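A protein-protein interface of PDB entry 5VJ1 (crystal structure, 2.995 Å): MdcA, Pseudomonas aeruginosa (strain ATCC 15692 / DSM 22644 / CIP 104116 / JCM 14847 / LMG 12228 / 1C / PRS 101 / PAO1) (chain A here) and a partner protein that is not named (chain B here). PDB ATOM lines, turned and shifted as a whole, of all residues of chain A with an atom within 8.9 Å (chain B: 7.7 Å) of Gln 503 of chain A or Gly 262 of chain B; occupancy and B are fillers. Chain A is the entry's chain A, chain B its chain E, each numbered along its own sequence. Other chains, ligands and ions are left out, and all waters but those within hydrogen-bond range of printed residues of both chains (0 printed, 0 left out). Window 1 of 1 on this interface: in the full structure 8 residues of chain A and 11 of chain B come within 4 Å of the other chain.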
ATOM      1  N   ALA A 486     -33.957  13.339   6.315  1.00  0.00           N
ATOM      2  CA  ALA A 486     -32.971  13.532   5.244  1.00  0.00           C
ATOM      3  C   ALA A 486     -32.619  12.216   4.527  1.00  0.00           C
ATOM      4  O   ALA A 486     -32.402  12.196   3.324  1.00  0.00           O
ATOM      5  CB  ALA A 486     -31.731  14.189   5.780  1.00  0.00           C
ATOM      6  N   HIS A 497     -38.561  16.596   4.803  1.00  0.00           N
ATOM      7  CA  HIS A 497     -37.253  17.168   4.560  1.00  0.00           C
ATOM      8  C   HIS A 497     -37.164  18.167   3.419  1.00  0.00           C
ATOM      9  O   HIS A 497     -37.565  17.863   2.291  1.00  0.00           O
ATOM     10  CB  HIS A 497     -36.264  16.044   4.304  1.00  0.00           C
ATOM     11  CG  HIS A 497     -34.881  16.532   4.039  1.00  0.00           C
ATOM     12  ND1 HIS A 497     -34.095  17.059   5.033  1.00  0.00           N
ATOM     13  CD2 HIS A 497     -34.165  16.592   2.900  1.00  0.00           C
ATOM     14  CE1 HIS A 497     -32.929  17.426   4.511  1.00  0.00           C
ATOM     15  NE2 HIS A 497     -32.951  17.149   3.215  1.00  0.00           N
ATOM     16  N   ASP A 498     -36.575  19.327   3.698  1.00  0.00           N
ATOM     17  CA  ASP A 498     -36.350  20.340   2.666  1.00  0.00           C
ATOM     18  C   ASP A 498     -34.950  20.173   2.071  1.00  0.00           C
ATOM     19  O   ASP A 498     -33.953  20.480   2.729  1.00  0.00           O
ATOM     20  CB  ASP A 498     -36.517  21.748   3.241  1.00  0.00           C
ATOM     21  CG  ASP A 498     -35.949  22.837   2.320  1.00  0.00           C
ATOM     22  OD1 ASP A 498     -35.805  22.593   1.101  1.00  0.00           O
ATOM     23  OD2 ASP A 498     -35.691  23.967   2.804  1.00  0.00           O
ATOM     24  N   PRO A 499     -34.872  19.734   0.805  1.00  0.00           N
ATOM     25  CA  PRO A 499     -33.629  19.407   0.093  1.00  0.00           C
ATOM     26  C   PRO A 499     -32.519  20.486   0.130  1.00  0.00           C
ATOM     27  O   PRO A 499     -31.339  20.138   0.028  1.00  0.00           O
ATOM     28  CB  PRO A 499     -34.115  19.164  -1.341  1.00  0.00           C
ATOM     29  CG  PRO A 499     -35.451  19.839  -1.418  1.00  0.00           C
ATOM     30  CD  PRO A 499     -36.038  19.568  -0.071  1.00  0.00           C
ATOM     31  N   ARG A 500     -32.863  21.764   0.212  1.00  0.00           N
ATOM     32  CA  ARG A 500     -31.836  22.794   0.229  1.00  0.00           C
ATOM     33  C   ARG A 500     -31.025  22.723   1.497  1.00  0.00           C
ATOM     34  O   ARG A 500     -29.936  23.298   1.581  1.00  0.00           O
ATOM     35  CB  ARG A 500     -32.458  24.177   0.151  1.00  0.00           C
ATOM     36  CG  ARG A 500     -33.697  24.295  -0.689  1.00  0.00           C
ATOM     37  CD  ARG A 500     -34.572  25.239   0.064  1.00  0.00           C
ATOM     38  NE  ARG A 500     -35.445  26.061  -0.741  1.00  0.00           N
ATOM     39  CZ  ARG A 500     -36.466  26.713  -0.212  1.00  0.00           C
ATOM     40  NH1 ARG A 500     -36.710  26.558   1.084  1.00  0.00           N
ATOM     41  NH2 ARG A 500     -37.249  27.477  -0.972  1.00  0.00           N
ATOM     42  N   GLU A 501     -31.552  21.983   2.470  1.00  0.00           N
ATOM     43  CA  GLU A 501     -30.894  21.782   3.753  1.00  0.00           C
ATOM     44  C   GLU A 501     -29.880  20.623   3.748  1.00  0.00           C
ATOM     45  O   GLU A 501     -29.139  20.426   4.729  1.00  0.00           O
ATOM     46  CB  GLU A 501     -31.938  21.529   4.841  1.00  0.00           C
ATOM     47  CG  GLU A 501     -32.717  22.738   5.316  1.00  0.00           C
ATOM     48  CD  GLU A 501     -31.835  23.918   5.682  1.00  0.00           C
ATOM     49  OE1 GLU A 501     -30.799  23.714   6.367  1.00  0.00           O
ATOM     50  OE2 GLU A 501     -32.216  25.063   5.328  1.00  0.00           O
ATOM     51  N   THR A 502     -29.842  19.854   2.659  1.00  0.00           N
ATOM     52  CA  THR A 502     -29.008  18.657   2.629  1.00  0.00           C
ATOM     53  C   THR A 502     -27.529  18.973   2.691  1.00  0.00           C
ATOM     54  O   THR A 502     -26.802  18.348   3.441  1.00  0.00           O
ATOM     55  CB  THR A 502     -29.264  17.812   1.380  1.00  0.00           C
ATOM     56  OG1 THR A 502     -30.638  17.419   1.355  1.00  0.00           O
ATOM     57  CG2 THR A 502     -28.418  16.564   1.435  1.00  0.00           C
ATOM     58  N   GLN A 503     -27.090  19.955   1.917  1.00  0.00           N
ATOM     59  CA  GLN A 503     -25.667  20.217   1.820  1.00  0.00           C
ATOM     60  C   GLN A 503     -25.154  20.516   3.229  1.00  0.00           C
ATOM     61  O   GLN A 503     -24.188  19.876   3.677  1.00  0.00           O
ATOM     62  CB  GLN A 503     -25.377  21.344   0.813  1.00  0.00           C
ATOM     63  CG  GLN A 503     -23.894  21.651   0.590  1.00  0.00           C
ATOM     64  CD  GLN A 503     -23.314  22.625   1.610  1.00  0.00           C
ATOM     65  OE1 GLN A 503     -24.039  23.291   2.355  1.00  0.00           O
ATOM     66  NE2 GLN A 503     -21.996  22.669   1.683  1.00  0.00           N
ATOM     67  N   ARG A 504     -25.837  21.419   3.945  1.00  0.00           N
ATOM     68  CA  ARG A 504     -25.507  21.747   5.337  1.00  0.00           C
ATOM     69  C   ARG A 504     -25.308  20.504   6.198  1.00  0.00           C
ATOM     70  O   ARG A 504     -24.334  20.373   6.940  1.00  0.00           O
ATOM     71  CB  ARG A 504     -26.627  22.583   5.946  1.00  0.00           C
ATOM     72  CG  ARG A 504     -26.426  23.000   7.374  1.00  0.00           C
ATOM     73  CD  ARG A 504     -26.255  24.486   7.415  1.00  0.00           C
ATOM     74  NE  ARG A 504     -25.423  24.901   8.533  1.00  0.00           N
ATOM     75  CZ  ARG A 504     -25.181  26.171   8.841  1.00  0.00           C
ATOM     76  NH1 ARG A 504     -25.709  27.151   8.107  1.00  0.00           N
ATOM     77  NH2 ARG A 504     -24.407  26.461   9.882  1.00  0.00           N
ATOM     78  N   MET A 505     -26.250  19.579   6.080  1.00  0.00           N
ATOM     79  CA  MET A 505     -26.255  18.388   6.915  1.00  0.00           C
ATOM     80  C   MET A 505     -25.120  17.463   6.518  1.00  0.00           C
ATOM     81  O   MET A 505     -24.618  16.693   7.352  1.00  0.00           O
ATOM     82  CB  MET A 505     -27.609  17.689   6.814  1.00  0.00           C
ATOM     83  CG  MET A 505     -28.747  18.538   7.348  1.00  0.00           C
ATOM     84  SD  MET A 505     -30.373  17.760   7.281  1.00  0.00           S
ATOM     85  CE  MET A 505     -30.311  16.646   8.670  1.00  0.00           C
ATOM     86  N   ARG A 506     -24.741  17.528   5.240  1.00  0.00           N
ATOM     87  CA  ARG A 506     -23.680  16.690   4.705  1.00  0.00           C
ATOM     88  C   ARG A 506     -22.344  17.200   5.180  1.00  0.00           C
ATOM     89  O   ARG A 506     -21.498  16.438   5.688  1.00  0.00           O
ATOM     90  CB  ARG A 506     -23.720  16.652   3.180  1.00  0.00           C
ATOM     91  CG  ARG A 506     -24.944  15.971   2.641  1.00  0.00           C
ATOM     92  CD  ARG A 506     -24.675  15.125   1.418  1.00  0.00           C
ATOM     93  NE  ARG A 506     -24.507  15.863   0.168  1.00  0.00           N
ATOM     94  CZ  ARG A 506     -23.662  15.495  -0.796  1.00  0.00           C
ATOM     95  NH1 ARG A 506     -22.918  14.412  -0.651  1.00  0.00           N
ATOM     96  NH2 ARG A 506     -23.549  16.202  -1.907  1.00  0.00           N
ATOM     97  N   ARG A 507     -22.172  18.503   5.018  1.00  0.00           N
ATOM     98  CA  ARG A 507     -20.945  19.170   5.400  1.00  0.00           C
ATOM     99  C   ARG A 507     -20.697  19.006   6.864  1.00  0.00           C
ATOM    100  O   ARG A 507     -19.576  18.705   7.271  1.00  0.00           O
ATOM    101  CB  ARG A 507     -21.017  20.651   5.048  1.00  0.00           C
ATOM    102  CG  ARG A 507     -19.796  21.436   5.429  1.00  0.00           C
ATOM    103  CD  ARG A 507     -19.865  22.814   4.818  1.00  0.00           C
ATOM    104  NE  ARG A 507     -21.048  23.559   5.242  1.00  0.00           N
ATOM    105  CZ  ARG A 507     -21.222  24.074   6.457  1.00  0.00           C
ATOM    106  NH1 ARG A 507     -20.291  23.907   7.398  1.00  0.00           N
ATOM    107  NH2 ARG A 507     -22.336  24.750   6.731  1.00  0.00           N
ATOM    108  N   GLU A 508     -21.755  19.161   7.659  1.00  0.00           N
ATOM    109  CA  GLU A 508     -21.619  19.076   9.106  1.00  0.00           C
ATOM    110  C   GLU A 508     -21.448  17.623   9.540  1.00  0.00           C
ATOM    111  O   GLU A 508     -21.125  17.351  10.697  1.00  0.00           O
ATOM    112  CB  GLU A 508     -22.820  19.722   9.814  1.00  0.00           C
ATOM    113  CG  GLU A 508     -22.828  21.247   9.786  1.00  0.00           C
ATOM    114  CD  GLU A 508     -24.013  21.856  10.534  1.00  0.00           C
ATOM    115  OE1 GLU A 508     -25.153  21.772  10.037  1.00  0.00           O
ATOM    116  OE2 GLU A 508     -23.819  22.393  11.643  1.00  0.00           O
ATOM    117  N   GLY A 509     -21.606  16.697   8.596  1.00  0.00           N
ATOM    118  CA  GLY A 509     -21.371  15.291   8.864  1.00  0.00           C
ATOM    119  C   GLY A 509     -22.507  14.676   9.644  1.00  0.00           C
ATOM    120  O   GLY A 509     -22.324  13.703  10.397  1.00  0.00           O
ATOM    121  N   LEU A 510     -23.682  15.285   9.495  1.00  0.00           N
ATOM    122  CA  LEU A 510     -24.873  14.804  10.165  1.00  0.00           C
ATOM    123  C   LEU A 510     -25.386  13.611   9.405  1.00  0.00           C
ATOM    124  O   LEU A 510     -25.815  12.619   9.987  1.00  0.00           O
ATOM    125  CB  LEU A 510     -25.921  15.899  10.253  1.00  0.00           C
ATOM    126  CG  LEU A 510     -25.549  17.046  11.183  1.00  0.00           C
ATOM    127  CD1 LEU A 510     -26.568  18.166  11.057  1.00  0.00           C
ATOM    128  CD2 LEU A 510     -25.494  16.519  12.599  1.00  0.00           C
ATOM    129  N   ILE A 511     -25.312  13.711   8.085  1.00  0.00           N
ATOM    130  CA  ILE A 511     -25.686  12.613   7.208  1.00  0.00           C
ATOM    131  C   ILE A 511     -24.529  12.359   6.264  1.00  0.00           C
ATOM    132  O   ILE A 511     -23.658  13.209   6.086  1.00  0.00           O
ATOM    133  CB  ILE A 511     -26.960  12.916   6.390  1.00  0.00           C
ATOM    134  CG1 ILE A 511     -26.741  14.172   5.551  1.00  0.00           C
ATOM    135  CG2 ILE A 511     -28.174  13.094   7.290  1.00  0.00           C
ATOM    136  CD1 ILE A 511     -27.817  14.437   4.530  1.00  0.00           C
ATOM    137  N   LEU A 513     -24.110  10.873   2.285  1.00  0.00           N
ATOM    138  CA  LEU A 513     -24.668  10.258   1.089  1.00  0.00           C
ATOM    139  C   LEU A 513     -23.642   9.266   0.562  1.00  0.00           C
ATOM    140  O   LEU A 513     -22.460   9.307   0.969  1.00  0.00           O
ATOM    141  CB  LEU A 513     -25.027  11.303   0.042  1.00  0.00           C
ATOM    142  CG  LEU A 513     -26.179  12.208   0.489  1.00  0.00           C
ATOM    143  CD1 LEU A 513     -26.660  13.047  -0.660  1.00  0.00           C
ATOM    144  CD2 LEU A 513     -27.331  11.439   1.115  1.00  0.00           C
ATOM    145  N   ASP A 516     -20.642  10.722  -0.453  1.00  0.00           N
ATOM    146  CA  ASP A 516     -19.808  11.265   0.632  1.00  0.00           C
ATOM    147  C   ASP A 516     -18.812  10.232   1.154  1.00  0.00           C
ATOM    148  O   ASP A 516     -17.826  10.565   1.838  1.00  0.00           O
ATOM    149  CB  ASP A 516     -20.684  11.748   1.786  1.00  0.00           C
ATOM    150  CG  ASP A 516     -21.320  13.106   1.520  1.00  0.00           C
ATOM    151  OD1 ASP A 516     -22.461  13.306   1.994  1.00  0.00           O
ATOM    152  OD2 ASP A 516     -20.708  13.956   0.835  1.00  0.00           O
ATOM    153  N   ARG B 142     -27.805  39.519  -1.689  1.00  0.00           N
ATOM    154  CA  ARG B 142     -28.130  38.096  -1.573  1.00  0.00           C
ATOM    155  C   ARG B 142     -28.319  37.692  -0.106  1.00  0.00           C
ATOM    156  O   ARG B 142     -29.266  36.959   0.249  1.00  0.00           O
ATOM    157  CB  ARG B 142     -27.016  37.252  -2.214  1.00  0.00           C
ATOM    158  CG  ARG B 142     -27.137  35.754  -1.981  1.00  0.00           C
ATOM    159  CD  ARG B 142     -26.076  34.947  -2.731  1.00  0.00           C
ATOM    160  NE  ARG B 142     -24.703  35.238  -2.319  1.00  0.00           N
ATOM    161  CZ  ARG B 142     -24.243  35.018  -1.089  1.00  0.00           C
ATOM    162  NH1 ARG B 142     -25.055  34.519  -0.164  1.00  0.00           N
ATOM    163  NH2 ARG B 142     -22.981  35.300  -0.764  1.00  0.00           N
ATOM    164  N   ASN B 169     -27.917  33.455  -6.239  1.00  0.00           N
ATOM    165  CA  ASN B 169     -28.477  32.344  -5.503  1.00  0.00           C
ATOM    166  C   ASN B 169     -28.661  31.154  -6.453  1.00  0.00           C
ATOM    167  O   ASN B 169     -28.581  30.001  -6.043  1.00  0.00           O
ATOM    168  CB  ASN B 169     -29.804  32.750  -4.851  1.00  0.00           C
ATOM    169  CG  ASN B 169     -29.624  33.336  -3.456  1.00  0.00           C
ATOM    170  OD1 ASN B 169     -29.836  34.533  -3.230  1.00  0.00           O
ATOM    171  ND2 ASN B 169     -29.259  32.476  -2.501  1.00  0.00           N
ATOM    172  N   ARG B 170     -28.916  31.443  -7.728  1.00  0.00           N
ATOM    173  CA  ARG B 170     -29.090  30.402  -8.742  1.00  0.00           C
ATOM    174  C   ARG B 170     -28.589  30.866 -10.110  1.00  0.00           C
ATOM    175  O   ARG B 170     -28.875  31.984 -10.548  1.00  0.00           O
ATOM    176  CB  ARG B 170     -30.554  29.983  -8.877  1.00  0.00           C
ATOM    177  CG  ARG B 170     -31.237  29.509  -7.621  1.00  0.00           C
ATOM    178  CD  ARG B 170     -30.805  28.137  -7.158  1.00  0.00           C
ATOM    179  NE  ARG B 170     -31.592  27.713  -5.998  1.00  0.00           N
ATOM    180  CZ  ARG B 170     -31.473  28.211  -4.773  1.00  0.00           C
ATOM    181  NH1 ARG B 170     -30.554  29.132  -4.514  1.00  0.00           N
ATOM    182  NH2 ARG B 170     -32.259  27.762  -3.800  1.00  0.00           N
ATOM    183  N   GLY B 221     -21.763  21.243 -12.057  1.00  0.00           N
ATOM    184  CA  GLY B 221     -22.958  21.392 -11.234  1.00  0.00           C
ATOM    185  C   GLY B 221     -23.040  22.769 -10.600  1.00  0.00           C
ATOM    186  O   GLY B 221     -23.358  22.908  -9.406  1.00  0.00           O
ATOM    187  N   PRO B 258     -31.978  28.683   2.393  1.00  0.00           N
ATOM    188  CA  PRO B 258     -30.608  29.125   2.649  1.00  0.00           C
ATOM    189  C   PRO B 258     -30.149  30.081   1.572  1.00  0.00           C
ATOM    190  O   PRO B 258     -30.472  29.914   0.385  1.00  0.00           O
ATOM    191  CB  PRO B 258     -29.824  27.831   2.601  1.00  0.00           C
ATOM    192  CG  PRO B 258     -30.799  26.833   3.128  1.00  0.00           C
ATOM    193  CD  PRO B 258     -32.090  27.219   2.471  1.00  0.00           C
ATOM    194  N   ARG B 259     -29.380  31.074   1.983  1.00  0.00           N
ATOM    195  CA  ARG B 259     -28.964  32.122   1.075  1.00  0.00           C
ATOM    196  C   ARG B 259     -27.528  31.945   0.586  1.00  0.00           C
ATOM    197  O   ARG B 259     -27.045  32.757  -0.209  1.00  0.00           O
ATOM    198  CB  ARG B 259     -29.116  33.468   1.771  1.00  0.00           C
ATOM    199  CG  ARG B 259     -30.502  33.695   2.289  1.00  0.00           C
ATOM    200  CD  ARG B 259     -30.542  34.839   3.261  1.00  0.00           C
ATOM    201  NE  ARG B 259     -31.914  35.276   3.501  1.00  0.00           N
ATOM    202  CZ  ARG B 259     -32.250  36.269   4.320  1.00  0.00           C
ATOM    203  NH1 ARG B 259     -31.306  36.938   4.974  1.00  0.00           N
ATOM    204  NH2 ARG B 259     -33.526  36.590   4.480  1.00  0.00           N
ATOM    205  N   ASP B 260     -26.847  30.902   1.077  1.00  0.00           N
ATOM    206  CA  ASP B 260     -25.438  30.689   0.745  1.00  0.00           C
ATOM    207  C   ASP B 260     -25.277  30.080  -0.621  1.00  0.00           C
ATOM    208  O   ASP B 260     -26.255  29.901  -1.345  1.00  0.00           O
ATOM    209  CB  ASP B 260     -24.728  29.836   1.807  1.00  0.00           C
ATOM    210  CG  ASP B 260     -25.562  28.646   2.287  1.00  0.00           C
ATOM    211  OD1 ASP B 260     -25.925  27.750   1.486  1.00  0.00           O
ATOM    212  OD2 ASP B 260     -25.872  28.623   3.503  1.00  0.00           O
ATOM    213  N   LEU B 261     -24.043  29.749  -0.969  1.00  0.00           N
ATOM    214  CA  LEU B 261     -23.785  29.182  -2.284  1.00  0.00           C
ATOM    215  C   LEU B 261     -23.579  27.663  -2.189  1.00  0.00           C
ATOM    216  O   LEU B 261     -22.976  27.032  -3.070  1.00  0.00           O
ATOM    217  CB  LEU B 261     -22.580  29.871  -2.906  1.00  0.00           C
ATOM    218  CG  LEU B 261     -22.691  31.383  -2.848  1.00  0.00           C
ATOM    219  CD1 LEU B 261     -21.520  32.009  -3.556  1.00  0.00           C
ATOM    220  CD2 LEU B 261     -23.950  31.739  -3.552  1.00  0.00           C
ATOM    221  N   GLY B 262     -24.131  27.089  -1.121  1.00  0.00           N
ATOM    222  CA  GLY B 262     -24.040  25.667  -0.858  1.00  0.00           C
ATOM    223  C   GLY B 262     -24.588  24.802  -1.968  1.00  0.00           C
ATOM    224  O   GLY B 262     -24.094  23.694  -2.164  1.00  0.00           O
ATOM    225  N   GLY B 263     -25.559  25.328  -2.719  1.00  0.00           N
ATOM    226  CA  GLY B 263     -26.176  24.609  -3.816  1.00  0.00           C
ATOM    227  C   GLY B 263     -25.222  24.279  -4.952  1.00  0.00           C
ATOM    228  O   GLY B 263     -25.543  23.486  -5.850  1.00  0.00           O
ATOM    229  N   ARG B 264     -24.039  24.886  -4.928  1.00  0.00           N
ATOM    230  CA  ARG B 264     -23.068  24.664  -5.987  1.00  0.00           C
ATOM    231  C   ARG B 264     -22.067  23.531  -5.683  1.00  0.00           C
ATOM    232  O   ARG B 264     -21.000  23.464  -6.288  1.00  0.00           O
ATOM    233  CB  ARG B 264     -22.320  25.964  -6.271  1.00  0.00           C
ATOM    234  CG  ARG B 264     -23.204  27.200  -6.414  1.00  0.00           C
ATOM    235  CD  ARG B 264     -22.348  28.447  -6.590  1.00  0.00           C
ATOM    236  NE  ARG B 264     -23.099  29.648  -6.956  1.00  0.00           N
ATOM    237  CZ  ARG B 264     -22.524  30.799  -7.301  1.00  0.00           C
ATOM    238  NH1 ARG B 264     -21.205  30.895  -7.354  1.00  0.00           N
ATOM    239  NH2 ARG B 264     -23.260  31.857  -7.606  1.00  0.00           N
ATOM    240  N   LEU B 265     -22.419  22.624  -4.776  1.00  0.00           N
ATOM    241  CA  LEU B 265     -21.508  21.543  -4.366  1.00  0.00           C
ATOM    242  C   LEU B 265     -22.038  20.134  -4.664  1.00  0.00           C
ATOM    243  O   LEU B 265     -21.469  19.129  -4.234  1.00  0.00           O
ATOM    244  CB  LEU B 265     -21.177  21.652  -2.870  1.00  0.00           C
ATOM    245  CG  LEU B 265     -20.379  22.857  -2.387  1.00  0.00           C
ATOM    246  CD1 LEU B 265     -20.142  22.711  -0.932  1.00  0.00           C
ATOM    247  CD2 LEU B 265     -19.050  22.883  -3.080  1.00  0.00           C
ATOM    248  N   GLY B 266     -23.144  20.053  -5.378  1.00  0.00           N
ATOM    249  CA  GLY B 266     -23.752  18.759  -5.603  1.00  0.00           C
ATOM    250  C   GLY B 266     -23.075  17.820  -6.587  1.00  0.00           C
ATOM    251  O   GLY B 266     -23.130  16.600  -6.401  1.00  0.00           O
ATOM    252  N   ARG B 270     -17.174  18.416  -8.684  1.00  0.00           N
ATOM    253  CA  ARG B 270     -16.722  19.231  -7.564  1.00  0.00           C
ATOM    254  C   ARG B 270     -16.600  18.382  -6.307  1.00  0.00           C
ATOM    255  O   ARG B 270     -16.627  18.930  -5.207  1.00  0.00           O
ATOM    256  CB  ARG B 270     -17.659  20.406  -7.291  1.00  0.00           C
ATOM    257  CG  ARG B 270     -17.669  21.494  -8.329  1.00  0.00           C
ATOM    258  CD  ARG B 270     -18.212  22.773  -7.734  1.00  0.00           C
ATOM    259  NE  ARG B 270     -17.173  23.558  -7.097  1.00  0.00           N
ATOM    260  CZ  ARG B 270     -17.392  24.682  -6.423  1.00  0.00           C
ATOM    261  NH1 ARG B 270     -18.619  25.150  -6.269  1.00  0.00           N
ATOM    262  NH2 ARG B 270     -16.378  25.339  -5.887  1.00  0.00           N
ATOM    263  N   SER B 273     -14.251  19.799  -3.674  1.00  0.00           N
ATOM    264  CA  SER B 273     -14.690  21.028  -3.028  1.00  0.00           C
ATOM    265  C   SER B 273     -15.517  20.700  -1.806  1.00  0.00           C
ATOM    266  O   SER B 273     -15.388  21.358  -0.782  1.00  0.00           O
ATOM    267  CB  SER B 273     -15.474  21.906  -3.988  1.00  0.00           C
ATOM    268  OG  SER B 273     -14.655  22.226  -5.093  1.00  0.00           O
ATOM    269  N   ALA B 274     -16.399  19.713  -1.947  1.00  0.00           N
ATOM    270  CA  ALA B 274     -17.272  19.276  -0.873  1.00  0.00           C
ATOM    271  C   ALA B 274     -16.499  18.565   0.224  1.00  0.00           C
ATOM    272  O   ALA B 274     -16.778  18.735   1.415  1.00  0.00           O
ATOM    273  CB  ALA B 274     -18.331  18.376  -1.415  1.00  0.00           C
ATOM    274  N   ARG B 277     -14.515  21.096   2.534  1.00  0.00           N
ATOM    275  CA  ARG B 277     -15.379  21.786   3.484  1.00  0.00           C
ATOM    276  C   ARG B 277     -15.741  20.867   4.630  1.00  0.00           C
ATOM    277  O   ARG B 277     -15.889  21.310   5.769  1.00  0.00           O
ATOM    278  CB  ARG B 277     -16.647  22.320   2.793  1.00  0.00           C
ATOM    279  CG  ARG B 277     -16.353  23.493   1.885  1.00  0.00           C
ATOM    280  CD  ARG B 277     -17.583  24.137   1.290  1.00  0.00           C
ATOM    281  NE  ARG B 277     -17.241  25.392   0.625  1.00  0.00           N
ATOM    282  CZ  ARG B 277     -16.716  25.478  -0.590  1.00  0.00           C
ATOM    283  NH1 ARG B 277     -16.486  24.381  -1.299  1.00  0.00           N
ATOM    284  NH2 ARG B 277     -16.434  26.666  -1.103  1.00  0.00           N
ATOM    285  N   ARG B 278     -15.867  19.580   4.329  1.00  0.00           N
ATOM    286  CA  ARG B 278     -16.218  18.601   5.347  1.00  0.00           C
ATOM    287  C   ARG B 278     -15.062  18.371   6.314  1.00  0.00           C
ATOM    288  O   ARG B 278     -15.253  18.404   7.527  1.00  0.00           O
ATOM    289  CB  ARG B 278     -16.653  17.288   4.694  1.00  0.00           C
ATOM    290  CG  ARG B 278     -16.829  16.152   5.663  1.00  0.00           C
ATOM    291  CD  ARG B 278     -17.814  15.162   5.082  1.00  0.00           C
ATOM    292  NE  ARG B 278     -17.553  14.824   3.682  1.00  0.00           N
ATOM    293  CZ  ARG B 278     -16.521  14.087   3.262  1.00  0.00           C
ATOM    294  NH1 ARG B 278     -15.623  13.593   4.156  1.00  0.00           N
ATOM    295  NH2 ARG B 278     -16.404  13.839   1.945  1.00  0.00           N
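Pro 258 of chain B touches Arg 500 of chain A (CD to CB, 3.8 Å).
CG of Pro 258 of chain B touches OE2 of Glu 501 of chain A (3.2 Å).
O of Gly 262 of chain B touches CG of Gln 503 of chain A (3.4 Å).
Gln 503 of chain A touches Leu 265 of chain B (NE2 to CD1, 3.2 Å).
Arg 506 of chain A touches Arg 278 of chain B (O to CD, 3.9 Å).
Arg 507 of chain A touches Arg 277 of chain B.
O of Arg 507 of chain A touches CA of Arg 278 of chain B, at 3.9 Å.
NH2 of Arg 278 of chain B touches O of Asp 516 of chain A (3.6 Å).
Printed residues of chain B within 4 Å of Glu 501 of chain A: Pro 258 (3.2 Å).
Of chain B, only Gly 262 and Leu 265 come within 4 Å of Gln 503 of chain A.
Of the printed residues of chain B, Arg 506 of chain A touches Arg 278.
Of the printed residues of chain B, Asp 516 of chain A touches Arg 278 (3.6 Å).
Arg 259 of chain B touches none of the printed residues of chain A.
Gly 262 of chain B touches just one residue of chain A: Gln 503.
No residue of chain A comes within 4 Å of Gly 263 of chain B.
The nearest residue of chain B that does not touch Gln 503 of chain A is Arg 277 of chain B (4.7 Å).
The nearest residue of chain A that does not touch Gly 262 of chain B is Arg 500 of chain A (6.6 Å).
Of the 18 printed residues of chain B, 5 touch a printed residue of chain A.
Printed residues of chain B that touch a printed residue of chain A: Pro 258, Gly 262, Leu 265, Arg 277 and Arg 278.
Among the printed residues, no Asp or Glu carboxylate lies within 4 Å of a Lys or Arg side-chain nitrogen of the other chain.
NH1 of Arg 500 of chain A is in salt-bridge range of OD2 of Asp 498 of chain A.
NH1 of Arg 506 of chain A is in salt-bridge range of OD2 of Asp 516 of chain A (2.7 Å).
N of Leu 513 of chain A sits at hydrogen-bond distance from OD1 of Asp 516 of chain A (3.0 Å).
The side-chain carboxylate of Asp 260 of chain B sits at hydrogen-bond distance from the backbone NH of Gly 262 of chain B.
The backbone carbonyl oxygen (O) of Ser 273 of chain B lies within hydrogen-bond range of the guanidinium group (NH1) of Arg 277 of chain B (3.3 Å).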
